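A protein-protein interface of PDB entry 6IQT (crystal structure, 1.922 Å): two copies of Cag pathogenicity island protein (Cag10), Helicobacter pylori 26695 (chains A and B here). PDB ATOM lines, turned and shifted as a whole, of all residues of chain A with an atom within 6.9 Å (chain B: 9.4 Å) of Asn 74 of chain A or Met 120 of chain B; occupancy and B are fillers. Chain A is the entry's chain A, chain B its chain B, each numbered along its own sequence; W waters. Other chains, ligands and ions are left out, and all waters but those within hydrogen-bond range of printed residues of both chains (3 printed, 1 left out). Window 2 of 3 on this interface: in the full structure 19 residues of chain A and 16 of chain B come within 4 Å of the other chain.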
ATOM      1  N   GLN A  66     -29.784   9.563  22.750  1.00  0.00           N
ATOM      2  CA  GLN A  66     -28.783   8.517  22.535  1.00  0.00           C
ATOM      3  C   GLN A  66     -28.085   8.651  21.187  1.00  0.00           C
ATOM      4  O   GLN A  66     -26.885   8.350  21.066  1.00  0.00           O
ATOM      5  CB  GLN A  66     -29.446   7.144  22.671  1.00  0.00           C
ATOM      6  CG  GLN A  66     -29.670   6.773  24.116  1.00  0.00           C
ATOM      7  CD  GLN A  66     -30.349   5.447  24.296  1.00  0.00           C
ATOM      8  OE1 GLN A  66     -31.004   4.942  23.389  1.00  0.00           O
ATOM      9  NE2 GLN A  66     -30.193   4.865  25.484  1.00  0.00           N
ATOM     10  N   THR A  67     -28.801   9.130  20.179  1.00  0.00           N
ATOM     11  CA  THR A  67     -28.198   9.293  18.863  1.00  0.00           C
ATOM     12  C   THR A  67     -27.100  10.343  18.879  1.00  0.00           C
ATOM     13  O   THR A  67     -26.020  10.135  18.314  1.00  0.00           O
ATOM     14  CB  THR A  67     -29.282   9.654  17.856  1.00  0.00           C
ATOM     15  OG1 THR A  67     -30.081   8.485  17.622  1.00  0.00           O
ATOM     16  CG2 THR A  67     -28.671  10.112  16.572  1.00  0.00           C
ATOM     17  N   GLN A  68     -27.344  11.477  19.532  1.00  0.00           N
ATOM     18  CA  GLN A  68     -26.313  12.506  19.590  1.00  0.00           C
ATOM     19  C   GLN A  68     -25.100  12.045  20.400  1.00  0.00           C
ATOM     20  O   GLN A  68     -23.951  12.322  20.026  1.00  0.00           O
ATOM     21  CB  GLN A  68     -26.917  13.791  20.164  1.00  0.00           C
ATOM     22  CG  GLN A  68     -25.925  14.916  20.354  1.00  0.00           C
ATOM     23  CD  GLN A  68     -25.348  15.416  19.052  1.00  0.00           C
ATOM     24  OE1 GLN A  68     -25.872  15.138  17.966  1.00  0.00           O
ATOM     25  NE2 GLN A  68     -24.254  16.148  19.147  1.00  0.00           N
ATOM     26  N   ALA A  69     -25.325  11.336  21.510  1.00  0.00           N
ATOM     27  CA  ALA A  69     -24.206  10.754  22.241  1.00  0.00           C
ATOM     28  C   ALA A  69     -23.396   9.817  21.351  1.00  0.00           C
ATOM     29  O   ALA A  69     -22.158   9.824  21.385  1.00  0.00           O
ATOM     30  CB  ALA A  69     -24.716  10.014  23.482  1.00  0.00           C
ATOM     31  N   MET A  70     -24.073   9.023  20.534  1.00  0.00           N
ATOM     32  CA  MET A  70     -23.375   8.102  19.637  1.00  0.00           C
ATOM     33  C   MET A  70     -22.557   8.854  18.561  1.00  0.00           C
ATOM     34  O   MET A  70     -21.448   8.434  18.210  1.00  0.00           O
ATOM     35  CB  MET A  70     -24.376   7.141  18.974  1.00  0.00           C
ATOM     36  CG  MET A  70     -23.693   6.023  18.201  1.00  0.00           C
ATOM     37  SD  MET A  70     -22.644   4.886  19.402  1.00  0.00           S
ATOM     38  CE  MET A  70     -23.198   3.157  18.788  1.00  0.00           C
ATOM     39  N   ARG A  71     -23.087   9.973  18.061  1.00  0.00           N
ATOM     40  CA  ARG A  71     -22.325  10.763  17.092  1.00  0.00           C
ATOM     41  C   ARG A  71     -21.040  11.304  17.708  1.00  0.00           C
ATOM     42  O   ARG A  71     -19.990  11.346  17.050  1.00  0.00           O
ATOM     43  CB  ARG A  71     -23.173  11.909  16.544  1.00  0.00           C
ATOM     44  CG  ARG A  71     -24.266  11.465  15.597  1.00  0.00           C
ATOM     45  CD  ARG A  71     -25.043  12.669  15.049  1.00  0.00           C
ATOM     46  NE  ARG A  71     -25.987  12.267  14.011  1.00  0.00           N
ATOM     47  CZ  ARG A  71     -25.687  12.186  12.718  1.00  0.00           C
ATOM     48  NH1 ARG A  71     -24.470  12.498  12.296  1.00  0.00           N
ATOM     49  NH2 ARG A  71     -26.609  11.796  11.842  1.00  0.00           N
ATOM     50  N   MET A  72     -21.089  11.710  18.975  1.00  0.00           N
ATOM     51  CA  MET A  72     -19.889  12.224  19.618  1.00  0.00           C
ATOM     52  C   MET A  72     -18.893  11.119  19.924  1.00  0.00           C
ATOM     53  O   MET A  72     -17.677  11.308  19.818  1.00  0.00           O
ATOM     54  CB  MET A  72     -20.267  12.973  20.897  1.00  0.00           C
ATOM     55  CG  MET A  72     -21.222  14.109  20.627  1.00  0.00           C
ATOM     56  SD  MET A  72     -21.717  15.020  22.247  1.00  0.00           S
ATOM     57  CE  MET A  72     -19.934  15.452  22.835  1.00  0.00           C
ATOM     58  N   PHE A  73     -19.427   9.970  20.333  1.00  0.00           N
ATOM     59  CA  PHE A  73     -18.602   8.784  20.526  1.00  0.00           C
ATOM     60  C   PHE A  73     -17.860   8.429  19.238  1.00  0.00           C
ATOM     61  O   PHE A  73     -16.642   8.213  19.245  1.00  0.00           O
ATOM     62  CB  PHE A  73     -19.507   7.640  21.002  1.00  0.00           C
ATOM     63  CG  PHE A  73     -18.821   6.303  21.163  1.00  0.00           C
ATOM     64  CD1 PHE A  73     -18.109   6.004  22.313  1.00  0.00           C
ATOM     65  CD2 PHE A  73     -18.953   5.322  20.191  1.00  0.00           C
ATOM     66  CE1 PHE A  73     -17.501   4.767  22.481  1.00  0.00           C
ATOM     67  CE2 PHE A  73     -18.350   4.080  20.351  1.00  0.00           C
ATOM     68  CZ  PHE A  73     -17.620   3.803  21.501  1.00  0.00           C
ATOM     69  N   ASN A  74     -18.586   8.392  18.112  1.00  0.00           N
ATOM     70  CA  ASN A  74     -17.969   8.017  16.836  1.00  0.00           C
ATOM     71  C   ASN A  74     -16.928   9.033  16.382  1.00  0.00           C
ATOM     72  O   ASN A  74     -15.935   8.657  15.744  1.00  0.00           O
ATOM     73  CB  ASN A  74     -19.037   7.849  15.752  1.00  0.00           C
ATOM     74  CG  ASN A  74     -19.848   6.570  15.920  1.00  0.00           C
ATOM     75  OD1 ASN A  74     -19.377   5.591  16.505  1.00  0.00           O
ATOM     76  ND2 ASN A  74     -21.073   6.577  15.423  1.00  0.00           N
ATOM     77  N   GLU A  75     -17.132  10.319  16.691  1.00  0.00           N
ATOM     78  CA  GLU A  75     -16.131  11.325  16.344  1.00  0.00           C
ATOM     79  C   GLU A  75     -14.819  11.098  17.100  1.00  0.00           C
ATOM     80  O   GLU A  75     -13.730  11.260  16.529  1.00  0.00           O
ATOM     81  CB  GLU A  75     -16.698  12.723  16.608  1.00  0.00           C
ATOM     82  CG  GLU A  75     -16.013  13.863  15.836  1.00  0.00           C
ATOM     83  CD  GLU A  75     -15.572  13.474  14.423  1.00  0.00           C
ATOM     84  OE1 GLU A  75     -14.401  13.748  14.074  1.00  0.00           O
ATOM     85  OE2 GLU A  75     -16.389  12.908  13.658  1.00  0.00           O
ATOM     86  N   ASN A  76     -14.891  10.699  18.379  1.00  0.00           N
ATOM     87  CA  ASN A  76     -13.662  10.357  19.103  1.00  0.00           C
ATOM     88  C   ASN A  76     -12.929   9.190  18.445  1.00  0.00           C
ATOM     89  O   ASN A  76     -11.691   9.183  18.362  1.00  0.00           O
ATOM     90  CB  ASN A  76     -13.964   9.993  20.566  1.00  0.00           C
ATOM     91  CG  ASN A  76     -14.391  11.187  21.417  1.00  0.00           C
ATOM     92  OD1 ASN A  76     -14.189  12.345  21.053  1.00  0.00           O
ATOM     93  ND2 ASN A  76     -14.983  10.895  22.569  1.00  0.00           N
ATOM     94  N   ILE A  77     -13.670   8.163  18.029  1.00  0.00           N
ATOM     95  CA  ILE A  77     -13.038   7.026  17.370  1.00  0.00           C
ATOM     96  C   ILE A  77     -12.298   7.493  16.127  1.00  0.00           C
ATOM     97  O   ILE A  77     -11.152   7.103  15.882  1.00  0.00           O
ATOM     98  CB  ILE A  77     -14.081   5.951  17.017  1.00  0.00           C
ATOM     99  CG1 ILE A  77     -14.833   5.495  18.270  1.00  0.00           C
ATOM    100  CG2 ILE A  77     -13.404   4.764  16.303  1.00  0.00           C
ATOM    101  CD1 ILE A  77     -15.874   4.448  17.997  1.00  0.00           C
ATOM    102  N   ARG A  78     -12.946   8.349  15.330  1.00  0.00           N
ATOM    103  CA  ARG A  78     -12.386   8.744  14.038  1.00  0.00           C
ATOM    104  C   ARG A  78     -11.065   9.480  14.195  1.00  0.00           C
ATOM    105  O   ARG A  78     -10.156   9.325  13.369  1.00  0.00           O
ATOM    106  CB  ARG A  78     -13.381   9.620  13.278  1.00  0.00           C
ATOM    107  CG  ARG A  78     -14.550   8.849  12.731  1.00  0.00           C
ATOM    108  CD  ARG A  78     -15.197   9.593  11.582  1.00  0.00           C
ATOM    109  NE  ARG A  78     -16.590   9.963  11.841  1.00  0.00           N
ATOM    110  CZ  ARG A  78     -17.593   9.104  12.017  1.00  0.00           C
ATOM    111  NH1 ARG A  78     -17.386   7.791  11.997  1.00  0.00           N
ATOM    112  NH2 ARG A  78     -18.815   9.562  12.231  1.00  0.00           N
ATOM    113  N   GLN A  79     -10.938  10.285  15.245  1.00  0.00           N
ATOM    114  CA  GLN A  79      -9.779  11.147  15.398  1.00  0.00           C
ATOM    115  C   GLN A  79      -8.680  10.543  16.259  1.00  0.00           C
ATOM    116  O   GLN A  79      -7.501  10.773  15.974  1.00  0.00           O
ATOM    117  CB  GLN A  79     -10.214  12.501  15.962  1.00  0.00           C
ATOM    118  CG  GLN A  79     -11.244  13.236  15.060  1.00  0.00           C
ATOM    119  CD  GLN A  79     -10.910  13.193  13.538  1.00  0.00           C
ATOM    120  OE1 GLN A  79      -9.738  13.150  13.142  1.00  0.00           O
ATOM    121  NE2 GLN A  79     -11.951  13.233  12.693  1.00  0.00           N
ATOM    122  N   LYS B  83     -36.655  15.550  14.051  1.00  0.00           N
ATOM    123  CA  LYS B  83     -35.373  15.001  14.498  1.00  0.00           C
ATOM    124  C   LYS B  83     -34.233  15.712  13.767  1.00  0.00           C
ATOM    125  O   LYS B  83     -33.593  15.169  12.873  1.00  0.00           O
ATOM    126  CB  LYS B  83     -35.333  13.501  14.227  1.00  0.00           C
ATOM    127  CG  LYS B  83     -36.077  12.631  15.242  1.00  0.00           C
ATOM    128  CD  LYS B  83     -35.591  11.199  15.111  1.00  0.00           C
ATOM    129  CE  LYS B  83     -34.964  10.664  16.396  1.00  0.00           C
ATOM    130  NZ  LYS B  83     -34.489   9.247  16.227  1.00  0.00           N
ATOM    131  N   THR B 116     -27.765  18.690  11.209  1.00  0.00           N
ATOM    132  CA  THR B 116     -27.636  17.240  11.148  1.00  0.00           C
ATOM    133  C   THR B 116     -28.949  16.570  11.526  1.00  0.00           C
ATOM    134  O   THR B 116     -29.639  17.032  12.445  1.00  0.00           O
ATOM    135  CB  THR B 116     -26.532  16.744  12.092  1.00  0.00           C
ATOM    136  OG1 THR B 116     -26.901  17.048  13.437  1.00  0.00           O
ATOM    137  CG2 THR B 116     -25.211  17.431  11.787  1.00  0.00           C
ATOM    138  N   PRO B 117     -29.334  15.502  10.832  1.00  0.00           N
ATOM    139  CA  PRO B 117     -30.497  14.735  11.281  1.00  0.00           C
ATOM    140  C   PRO B 117     -30.198  14.172  12.661  1.00  0.00           C
ATOM    141  O   PRO B 117     -29.068  13.764  12.956  1.00  0.00           O
ATOM    142  CB  PRO B 117     -30.632  13.630  10.225  1.00  0.00           C
ATOM    143  CG  PRO B 117     -29.267  13.468   9.684  1.00  0.00           C
ATOM    144  CD  PRO B 117     -28.615  14.825   9.737  1.00  0.00           C
ATOM    145  N   ASP B 118     -31.188  14.226  13.532  1.00  0.00           N
ATOM    146  CA  ASP B 118     -31.014  13.647  14.866  1.00  0.00           C
ATOM    147  C   ASP B 118     -31.318  12.153  14.801  1.00  0.00           C
ATOM    148  O   ASP B 118     -32.110  11.608  15.567  1.00  0.00           O
ATOM    149  CB  ASP B 118     -31.891  14.372  15.887  1.00  0.00           C
ATOM    150  CG  ASP B 118     -31.498  14.065  17.351  1.00  0.00           C
ATOM    151  OD1 ASP B 118     -30.287  13.982  17.680  1.00  0.00           O
ATOM    152  OD2 ASP B 118     -32.419  13.924  18.185  1.00  0.00           O
ATOM    153  N   THR B 119     -30.678  11.496  13.827  1.00  0.00           N
ATOM    154  CA  THR B 119     -30.799  10.069  13.538  1.00  0.00           C
ATOM    155  C   THR B 119     -29.396   9.552  13.241  1.00  0.00           C
ATOM    156  O   THR B 119     -28.425  10.313  13.239  1.00  0.00           O
ATOM    157  CB  THR B 119     -31.723   9.795  12.336  1.00  0.00           C
ATOM    158  OG1 THR B 119     -31.141  10.346  11.141  1.00  0.00           O
ATOM    159  CG2 THR B 119     -33.111  10.393  12.528  1.00  0.00           C
ATOM    160  N   MET B 120     -29.271   8.260  12.964  1.00  0.00           N
ATOM    161  CA  MET B 120     -27.939   7.735  12.643  1.00  0.00           C
ATOM    162  C   MET B 120     -27.600   7.915  11.150  1.00  0.00           C
ATOM    163  O   MET B 120     -26.595   7.397  10.677  1.00  0.00           O
ATOM    164  CB  MET B 120     -27.820   6.251  13.038  1.00  0.00           C
ATOM    165  CG  MET B 120     -27.533   5.997  14.531  1.00  0.00           C
ATOM    166  SD  MET B 120     -26.346   7.315  15.367  1.00  0.00           S
ATOM    167  CE  MET B 120     -24.622   6.825  14.588  1.00  0.00           C
ATOM    168  N   GLU B 121     -28.411   8.679  10.421  1.00  0.00           N
ATOM    169  CA  GLU B 121     -28.213   8.832   8.979  1.00  0.00           C
ATOM    170  C   GLU B 121     -26.929   9.586   8.634  1.00  0.00           C
ATOM    171  O   GLU B 121     -26.491  10.500   9.339  1.00  0.00           O
ATOM    172  CB  GLU B 121     -29.402   9.553   8.348  1.00  0.00           C
ATOM    173  CG  GLU B 121     -30.693   8.770   8.417  1.00  0.00           C
ATOM    174  CD  GLU B 121     -31.892   9.633   8.074  1.00  0.00           C
ATOM    175  OE1 GLU B 121     -32.330   9.586   6.903  1.00  0.00           O
ATOM    176  OE2 GLU B 121     -32.373  10.375   8.971  1.00  0.00           O
ATOM    177  N   ASN B 122     -26.376   9.249   7.477  1.00  0.00           N
ATOM    178  CA  ASN B 122     -25.057   9.723   7.081  1.00  0.00           C
ATOM    179  C   ASN B 122     -25.186  10.905   6.111  1.00  0.00           C
ATOM    180  O   ASN B 122     -24.947  10.790   4.908  1.00  0.00           O
ATOM    181  CB  ASN B 122     -24.267   8.558   6.471  1.00  0.00           C
ATOM    182  CG  ASN B 122     -22.934   8.992   5.873  1.00  0.00           C
ATOM    183  OD1 ASN B 122     -22.301   9.928   6.357  1.00  0.00           O
ATOM    184  ND2 ASN B 122     -22.515   8.318   4.803  1.00  0.00           N
ATOM    185  N   TYR B 123     -25.588  12.058   6.651  1.00  0.00           N
ATOM    186  CA  TYR B 123     -25.538  13.297   5.872  1.00  0.00           C
ATOM    187  C   TYR B 123     -25.632  14.493   6.812  1.00  0.00           C
ATOM    188  O   TYR B 123     -26.094  14.381   7.949  1.00  0.00           O
ATOM    189  CB  TYR B 123     -26.639  13.361   4.788  1.00  0.00           C
ATOM    190  CG  TYR B 123     -28.044  13.568   5.300  1.00  0.00           C
ATOM    191  CD1 TYR B 123     -28.561  14.849   5.489  1.00  0.00           C
ATOM    192  CD2 TYR B 123     -28.859  12.475   5.597  1.00  0.00           C
ATOM    193  CE1 TYR B 123     -29.875  15.031   5.975  1.00  0.00           C
ATOM    194  CE2 TYR B 123     -30.158  12.646   6.083  1.00  0.00           C
ATOM    195  CZ  TYR B 123     -30.663  13.927   6.258  1.00  0.00           C
ATOM    196  OH  TYR B 123     -31.965  14.085   6.715  1.00  0.00           O
HETATM  197  O   HOH W   1     -27.674  13.253  16.424  1.00  0.00           O
HETATM  198  O   HOH W   2     -24.300  13.083   9.712  1.00  0.00           O
HETATM  199  O   HOH W   3     -30.117  12.220  19.887  1.00  0.00           O
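Hydrophobic or aromatic side chains of chain A within 4 Å of the printed part of chain B: Met 70.
Hydrophobic or aromatic side chains of chain B that line the printed part of chain A: Pro 117 and Met 120.
Along chain B the printed residues that touch a printed residue of chain A span positions 117 to 121.
Among the printed residues, no Asp or Glu carboxylate lies within 4 Å of a Lys or Arg side-chain nitrogen of the other chain.
No position is printed for both chains.
Water W2 lies within hydrogen-bond range of the guanidinium group (NH1) of Arg 71 of chain A, the backbone carbonyl oxygen (O) of Tyr 123 of chain B and the backbone carbonyl oxygen (O) of Glu 121 of chain B.
Water W3 lies within hydrogen-bond range of the side-chain carboxylate (OD1) of Asp 118 of chain B (2.8 Å), the backbone NH (N) of Gln 68 of chain A (2.9 Å) and the backbone NH (N) of Thr 67 of chain A (3.4 Å).
Water W1 lies within hydrogen-bond range of the side-chain carboxylate of Asp 118 of chain B (3.0 Å), the side-chain amide oxygen of Gln 68 of chain A (3.0 Å) and the guanidinium group of Arg 71 of chain A (3.1 Å).
Of the printed residues of chain B, Thr 67 of chain A touches Asp 118, Thr 119 and Met 120.
Of the printed residues of chain B, Arg 71 of chain A touches Pro 117, Thr 119 and Glu 121.
Of chain B, only Met 120 (3.7 Å) comes within 4 Å of Asn 74 of chain A.
No residue of chain B comes within 4 Å of Ile 77 of chain A.
Of the printed residues of chain A, Asp 118 of chain B touches Thr 67.
Of the printed residues of chain A, Thr 119 of chain B touches Thr 67 and Arg 71.
Of chain A, only Thr 67 (3.8 Å), Met 70 (3.8 Å) and Asn 74 (3.7 Å) come within 4 Å of Met 120 of chain B.
The nearest residue of chain A that does not touch Met 120 of chain B is Arg 71 of chain A (4.1 Å).
Among the printed residues, merely in contact across the chains: Thr 67 of chain A with Asp 118 of chain B, Thr 67 of chain A with Thr 119 of chain B, Thr 67 of chain A with Met 120 of chain B, Met 70 of chain A with Met 120 of chain B and Asn 74 of chain A with Met 120 of chain B.
The backbone NH of Asp 118 of chain B sits at hydrogen-bond distance from the backbone carbonyl oxygen of Lys 83 of chain B, 2.7 Å away.
The side-chain carboxylate (OE2) of Glu 121 of chain B lies within hydrogen-bond range of the side-chain hydroxyl (OG1) of Thr 119 of chain B, at 2.5 Å.
The side-chain amide nitrogen (ND2) of Asn 74 of chain A sits close to the backbone carbonyl oxygen (O) of Met 70 of chain A (3.4 Å).
The backbone carbonyl oxygen (O) of Pro 117 of chain B sits at hydrogen-bond distance from the guanidinium group (NH2) of Arg 71 of chain A (3.3 Å).
The guanidinium group (NH2) of Arg 71 of chain A lies within hydrogen-bond range of the backbone carbonyl oxygen (O) of Glu 121 of chain B (2.8 Å).
NH2 of Arg 71 of chain A sits at hydrogen-bond distance from O of Thr 119 of chain B (2.7 Å).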
